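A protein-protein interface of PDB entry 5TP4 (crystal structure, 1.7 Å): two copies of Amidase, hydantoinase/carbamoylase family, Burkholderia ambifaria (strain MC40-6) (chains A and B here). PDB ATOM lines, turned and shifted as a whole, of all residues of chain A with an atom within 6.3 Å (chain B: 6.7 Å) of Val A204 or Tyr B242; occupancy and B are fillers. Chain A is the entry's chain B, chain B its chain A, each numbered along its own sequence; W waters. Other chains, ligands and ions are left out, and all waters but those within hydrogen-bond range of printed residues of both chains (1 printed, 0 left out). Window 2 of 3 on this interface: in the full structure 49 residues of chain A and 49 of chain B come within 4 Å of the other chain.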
ATOM      1  N   GLU A 200       0.826   0.303 -10.230  1.00  0.00           N
ATOM      2  CA  GLU A 200       1.763   0.202  -9.103  1.00  0.00           C
ATOM      3  C   GLU A 200       1.074  -0.031  -7.759  1.00  0.00           C
ATOM      4  O   GLU A 200       1.626  -0.717  -6.888  1.00  0.00           O
ATOM      5  CB  GLU A 200       2.594   1.476  -9.004  1.00  0.00           C
ATOM      6  CG  GLU A 200       3.558   1.426  -7.826  1.00  0.00           C
ATOM      7  CD  GLU A 200       4.249   2.737  -7.590  1.00  0.00           C
ATOM      8  OE1 GLU A 200       4.728   2.972  -6.455  1.00  0.00           O
ATOM      9  OE2 GLU A 200       4.298   3.532  -8.549  1.00  0.00           O
ATOM     10  N   GLY A 202       1.015   2.226  -5.636  1.00  0.00           N
ATOM     11  CA  GLY A 202       1.875   3.008  -4.773  1.00  0.00           C
ATOM     12  C   GLY A 202       2.210   4.300  -5.495  1.00  0.00           C
ATOM     13  O   GLY A 202       1.817   4.509  -6.644  1.00  0.00           O
ATOM     14  N   PRO A 203       2.947   5.194  -4.838  1.00  0.00           N
ATOM     15  CA  PRO A 203       3.158   6.554  -5.364  1.00  0.00           C
ATOM     16  C   PRO A 203       4.453   6.777  -6.129  1.00  0.00           C
ATOM     17  O   PRO A 203       4.652   7.895  -6.630  1.00  0.00           O
ATOM     18  CB  PRO A 203       3.160   7.380  -4.069  1.00  0.00           C
ATOM     19  CG  PRO A 203       3.893   6.426  -3.091  1.00  0.00           C
ATOM     20  CD  PRO A 203       3.528   5.016  -3.490  1.00  0.00           C
ATOM     21  N   VAL A 204       5.330   5.770  -6.229  1.00  0.00           N
ATOM     22  CA  VAL A 204       6.707   6.022  -6.666  1.00  0.00           C
ATOM     23  C   VAL A 204       6.766   6.434  -8.131  1.00  0.00           C
ATOM     24  O   VAL A 204       7.411   7.427  -8.489  1.00  0.00           O
ATOM     25  CB  VAL A 204       7.587   4.783  -6.423  1.00  0.00           C
ATOM     26  CG1 VAL A 204       8.963   5.027  -7.037  1.00  0.00           C
ATOM     27  CG2 VAL A 204       7.667   4.483  -4.943  1.00  0.00           C
ATOM     28  N   LEU A 205       6.149   5.650  -9.017  1.00  0.00           N
ATOM     29  CA  LEU A 205       6.305   5.967 -10.431  1.00  0.00           C
ATOM     30  C   LEU A 205       5.640   7.298 -10.764  1.00  0.00           C
ATOM     31  O   LEU A 205       6.190   8.102 -11.531  1.00  0.00           O
ATOM     32  CB  LEU A 205       5.724   4.840 -11.285  1.00  0.00           C
ATOM     33  CG  LEU A 205       6.327   3.458 -11.018  1.00  0.00           C
ATOM     34  CD1 LEU A 205       5.538   2.381 -11.805  1.00  0.00           C
ATOM     35  CD2 LEU A 205       7.793   3.457 -11.421  1.00  0.00           C
ATOM     36  N   GLU A 206       4.453   7.546 -10.198  1.00  0.00           N
ATOM     37  CA  GLU A 206       3.767   8.803 -10.473  1.00  0.00           C
ATOM     38  C   GLU A 206       4.566   9.987  -9.941  1.00  0.00           C
ATOM     39  O   GLU A 206       4.711  11.004 -10.628  1.00  0.00           O
ATOM     40  CB  GLU A 206       2.360   8.769  -9.867  1.00  0.00           C
ATOM     41  CG  GLU A 206       1.398   9.774 -10.481  1.00  0.00           C
ATOM     42  CD  GLU A 206       1.370  11.048  -9.715  1.00  0.00           C
ATOM     43  OE1 GLU A 206       1.735  11.014  -8.521  1.00  0.00           O
ATOM     44  OE2 GLU A 206       0.995  12.089 -10.298  1.00  0.00           O
ATOM     45  N   ALA A 207       5.131   9.850  -8.737  1.00  0.00           N
ATOM     46  CA  ALA A 207       5.895  10.937  -8.133  1.00  0.00           C
ATOM     47  C   ALA A 207       7.171  11.232  -8.908  1.00  0.00           C
ATOM     48  O   ALA A 207       7.619  12.382  -8.945  1.00  0.00           O
ATOM     49  CB  ALA A 207       6.224  10.595  -6.686  1.00  0.00           C
ATOM     50  N   ASN A 208       7.776  10.223  -9.517  1.00  0.00           N
ATOM     51  CA  ASN A 208       9.017  10.392 -10.265  1.00  0.00           C
ATOM     52  C   ASN A 208       8.813  10.664 -11.746  1.00  0.00           C
ATOM     53  O   ASN A 208       9.801  10.867 -12.459  1.00  0.00           O
ATOM     54  CB  ASN A 208       9.888   9.138 -10.113  1.00  0.00           C
ATOM     55  CG  ASN A 208      10.522   9.052  -8.756  1.00  0.00           C
ATOM     56  OD1 ASN A 208      10.708  10.073  -8.100  1.00  0.00           O
ATOM     57  ND2 ASN A 208      10.866   7.842  -8.321  1.00  0.00           N
ATOM     58  N   GLY A 209       7.578  10.649 -12.239  1.00  0.00           N
ATOM     59  CA  GLY A 209       7.407  10.731 -13.674  1.00  0.00           C
ATOM     60  C   GLY A 209       7.941   9.517 -14.403  1.00  0.00           C
ATOM     61  O   GLY A 209       8.346   9.621 -15.562  1.00  0.00           O
ATOM     62  N   THR A 210       7.944   8.354 -13.757  1.00  0.00           N
ATOM     63  CA  THR A 210       8.437   7.145 -14.385  1.00  0.00           C
ATOM     64  C   THR A 210       7.270   6.410 -15.016  1.00  0.00           C
ATOM     65  O   THR A 210       6.286   6.119 -14.333  1.00  0.00           O
ATOM     66  CB  THR A 210       9.105   6.224 -13.365  1.00  0.00           C
ATOM     67  OG1 THR A 210      10.054   6.968 -12.599  1.00  0.00           O
ATOM     68  CG2 THR A 210       9.798   5.111 -14.076  1.00  0.00           C
ATOM     69  N   GLU A 358      12.216   2.522 -14.039  1.00  0.00           N
ATOM     70  CA  GLU A 358      13.042   2.266 -12.865  1.00  0.00           C
ATOM     71  C   GLU A 358      12.697   0.904 -12.289  1.00  0.00           C
ATOM     72  O   GLU A 358      11.565   0.420 -12.410  1.00  0.00           O
ATOM     73  CB  GLU A 358      12.890   3.349 -11.788  1.00  0.00           C
ATOM     74  CG  GLU A 358      11.552   3.413 -11.065  1.00  0.00           C
ATOM     75  CD  GLU A 358      11.446   4.659 -10.156  1.00  0.00           C
ATOM     76  OE1 GLU A 358      11.922   4.602  -8.998  1.00  0.00           O
ATOM     77  OE2 GLU A 358      10.910   5.698 -10.605  1.00  0.00           O
ATOM     78  N   ILE A 360      11.695  -1.499  -9.341  1.00  0.00           N
ATOM     79  CA  ILE A 360      10.802  -1.252  -8.211  1.00  0.00           C
ATOM     80  C   ILE A 360      10.333  -2.594  -7.667  1.00  0.00           C
ATOM     81  O   ILE A 360      10.177  -3.558  -8.411  1.00  0.00           O
ATOM     82  CB  ILE A 360       9.613  -0.377  -8.690  1.00  0.00           C
ATOM     83  CG1 ILE A 360       8.664  -0.022  -7.542  1.00  0.00           C
ATOM     84  CG2 ILE A 360       8.818  -1.109  -9.792  1.00  0.00           C
ATOM     85  CD1 ILE A 360       7.765   1.200  -7.895  1.00  0.00           C
ATOM     86  N   VAL B 231      -2.176  10.186   5.996  1.00  0.00           N
ATOM     87  CA  VAL B 231      -2.615   9.553   4.752  1.00  0.00           C
ATOM     88  C   VAL B 231      -2.560   8.040   4.950  1.00  0.00           C
ATOM     89  O   VAL B 231      -1.485   7.486   5.214  1.00  0.00           O
ATOM     90  CB  VAL B 231      -1.752   9.980   3.556  1.00  0.00           C
ATOM     91  CG1 VAL B 231      -2.121   9.169   2.297  1.00  0.00           C
ATOM     92  CG2 VAL B 231      -1.922  11.455   3.308  1.00  0.00           C
ATOM     93  N   ALA B 233      -2.110   4.958   3.567  1.00  0.00           N
ATOM     94  CA  ALA B 233      -1.566   4.359   2.366  1.00  0.00           C
ATOM     95  C   ALA B 233      -1.095   2.942   2.689  1.00  0.00           C
ATOM     96  O   ALA B 233      -1.035   2.530   3.851  1.00  0.00           O
ATOM     97  CB  ALA B 233      -0.429   5.222   1.802  1.00  0.00           C
ATOM     98  N   THR B 237       3.512  -0.801  -0.359  1.00  0.00           N
ATOM     99  CA  THR B 237       3.769  -0.107  -1.619  1.00  0.00           C
ATOM    100  C   THR B 237       4.287   1.308  -1.426  1.00  0.00           C
ATOM    101  O   THR B 237       4.630   1.953  -2.420  1.00  0.00           O
ATOM    102  CB  THR B 237       2.510  -0.003  -2.489  1.00  0.00           C
ATOM    103  OG1 THR B 237       1.572   0.855  -1.828  1.00  0.00           O
ATOM    104  CG2 THR B 237       1.863  -1.359  -2.734  1.00  0.00           C
ATOM    105  N   THR B 238       4.298   1.816  -0.193  1.00  0.00           N
ATOM    106  CA  THR B 238       4.561   3.232   0.083  1.00  0.00           C
ATOM    107  C   THR B 238       5.917   3.344   0.762  1.00  0.00           C
ATOM    108  O   THR B 238       6.033   3.018   1.950  1.00  0.00           O
ATOM    109  CB  THR B 238       3.472   3.816   0.990  1.00  0.00           C
ATOM    110  OG1 THR B 238       2.166   3.478   0.479  1.00  0.00           O
ATOM    111  CG2 THR B 238       3.617   5.348   1.083  1.00  0.00           C
ATOM    112  N   PRO B 239       6.967   3.780   0.071  1.00  0.00           N
ATOM    113  CA  PRO B 239       8.260   3.958   0.736  1.00  0.00           C
ATOM    114  C   PRO B 239       8.173   4.999   1.845  1.00  0.00           C
ATOM    115  O   PRO B 239       7.313   5.885   1.840  1.00  0.00           O
ATOM    116  CB  PRO B 239       9.178   4.424  -0.400  1.00  0.00           C
ATOM    117  CG  PRO B 239       8.516   3.892  -1.633  1.00  0.00           C
ATOM    118  CD  PRO B 239       7.061   4.035  -1.374  1.00  0.00           C
ATOM    119  N   MET B 240       9.093   4.872   2.808  1.00  0.00           N
ATOM    120  CA  MET B 240       9.036   5.735   3.985  1.00  0.00           C
ATOM    121  C   MET B 240       9.004   7.222   3.653  1.00  0.00           C
ATOM    122  O   MET B 240       8.224   7.938   4.301  1.00  0.00           O
ATOM    123  CB  MET B 240      10.193   5.407   4.942  1.00  0.00           C
ATOM    124  CG  MET B 240      10.204   3.931   5.398  1.00  0.00           C
ATOM    125  SD  MET B 240       8.730   3.357   6.273  1.00  0.00           S
ATOM    126  CE  MET B 240       8.912   4.269   7.827  1.00  0.00           C
ATOM    127  N   PRO B 241       9.784   7.753   2.700  1.00  0.00           N
ATOM    128  CA  PRO B 241       9.766   9.216   2.483  1.00  0.00           C
ATOM    129  C   PRO B 241       8.440   9.768   1.987  1.00  0.00           C
ATOM    130  O   PRO B 241       8.204  10.978   2.124  1.00  0.00           O
ATOM    131  CB  PRO B 241      10.868   9.424   1.440  1.00  0.00           C
ATOM    132  CG  PRO B 241      11.802   8.289   1.652  1.00  0.00           C
ATOM    133  CD  PRO B 241      10.895   7.122   1.961  1.00  0.00           C
ATOM    134  N   TYR B 242       7.559   8.932   1.431  1.00  0.00           N
ATOM    135  CA  TYR B 242       6.249   9.369   0.959  1.00  0.00           C
ATOM    136  C   TYR B 242       5.188   9.406   2.041  1.00  0.00           C
ATOM    137  O   TYR B 242       4.074   9.861   1.772  1.00  0.00           O
ATOM    138  CB  TYR B 242       5.756   8.447  -0.148  1.00  0.00           C
ATOM    139  CG  TYR B 242       6.631   8.460  -1.366  1.00  0.00           C
ATOM    140  CD1 TYR B 242       7.775   7.680  -1.416  1.00  0.00           C
ATOM    141  CD2 TYR B 242       6.322   9.255  -2.460  1.00  0.00           C
ATOM    142  CE1 TYR B 242       8.592   7.679  -2.518  1.00  0.00           C
ATOM    143  CE2 TYR B 242       7.148   9.256  -3.583  1.00  0.00           C
ATOM    144  CZ  TYR B 242       8.281   8.462  -3.591  1.00  0.00           C
ATOM    145  OH  TYR B 242       9.122   8.432  -4.684  1.00  0.00           O
ATOM    146  N   ARG B 243       5.483   8.909   3.233  1.00  0.00           N
ATOM    147  CA  ARG B 243       4.440   8.647   4.207  1.00  0.00           C
ATOM    148  C   ARG B 243       4.091   9.875   5.023  1.00  0.00           C
ATOM    149  O   ARG B 243       4.929  10.747   5.279  1.00  0.00           O
ATOM    150  CB  ARG B 243       4.869   7.539   5.170  1.00  0.00           C
ATOM    151  CG  ARG B 243       5.129   6.234   4.447  1.00  0.00           C
ATOM    152  CD  ARG B 243       5.534   5.160   5.390  1.00  0.00           C
ATOM    153  NE  ARG B 243       5.637   3.916   4.622  1.00  0.00           N
ATOM    154  CZ  ARG B 243       5.414   2.715   5.122  1.00  0.00           C
ATOM    155  NH1 ARG B 243       5.096   2.584   6.400  1.00  0.00           N
ATOM    156  NH2 ARG B 243       5.517   1.645   4.329  1.00  0.00           N
ATOM    157  N   LYS B 244       2.829   9.904   5.454  1.00  0.00           N
ATOM    158  CA  LYS B 244       2.290  10.889   6.389  1.00  0.00           C
ATOM    159  C   LYS B 244       1.622  10.050   7.477  1.00  0.00           C
ATOM    160  O   LYS B 244       0.405   9.865   7.514  1.00  0.00           O
ATOM    161  CB  LYS B 244       1.353  11.837   5.672  1.00  0.00           C
ATOM    162  CG  LYS B 244       2.106  12.691   4.652  1.00  0.00           C
ATOM    163  CD  LYS B 244       1.177  13.627   3.912  1.00  0.00           C
ATOM    164  CE  LYS B 244       1.923  14.465   2.890  1.00  0.00           C
ATOM    165  NZ  LYS B 244       0.958  15.124   1.963  1.00  0.00           N
ATOM    166  N   ILE B 285      -1.053   2.210   6.575  1.00  0.00           N
ATOM    167  CA  ILE B 285      -0.510   3.277   7.408  1.00  0.00           C
ATOM    168  C   ILE B 285      -1.647   4.015   8.100  1.00  0.00           C
ATOM    169  O   ILE B 285      -2.684   4.278   7.488  1.00  0.00           O
ATOM    170  CB  ILE B 285       0.306   4.230   6.520  1.00  0.00           C
ATOM    171  CG1 ILE B 285       1.520   3.496   5.927  1.00  0.00           C
ATOM    172  CG2 ILE B 285       0.682   5.517   7.278  1.00  0.00           C
ATOM    173  CD1 ILE B 285       2.095   4.188   4.683  1.00  0.00           C
HETATM  174  O   HOH W   1       5.388   1.019  -4.852  1.00  0.00           O
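Val A204 touches just these residues of chain B: Pro B239 (3.5 Å) and Tyr B242 (3.9 Å).
Of chain A, only Pro A203, Val A204 and Ala A207 come within 4 Å of Tyr B242.
Of the printed residues of chain A, Thr B237 touches Gly A202 and Pro A203.
Printed residues of chain B within 4 Å of Pro A203: Thr B237 (3.4 Å) and Tyr B242 (3.8 Å).
Of the printed residues of chain B, Ala A207 touches Tyr B242 (3.5 Å).
The side-chain carboxylate (OE1) of Glu A200 is in hydrogen-bond range of the backbone NH (N) of Val A204 (2.9 Å).
The backbone carbonyl oxygen (O) of Val A204 lies close to the side-chain amide nitrogen (ND2) of Asn A208 (3.5 Å).
Gly A202 touches Thr B237 (CA to OG1, 3.7 Å).
Thr B237 touches Pro A203.
CD2 of Tyr B242 touches CG of Pro A203 (3.8 Å).
CG of Pro B239 touches CG2 of Val A204, 3.5 Å away.
OH of Tyr B242 touches CA of Val A204, at 3.9 Å.
Ala A207 touches Tyr B242 (CB to CE2, 3.5 Å).
Water W1 bridges OE1 of Glu A200 and O of Thr B237.
No position is printed for both chains.
Of the 6 pairs that touch across the chains among the printed residues, none has its exchanged pair printed and touching as well.
Of the 11 printed residues of chain B, 3 touch a printed residue of chain A.
Printed residues of chain B that touch a printed residue of chain A: Thr B237, Pro B239 and Tyr B242.
Among the printed residues, 6 pairs touch across the chains.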
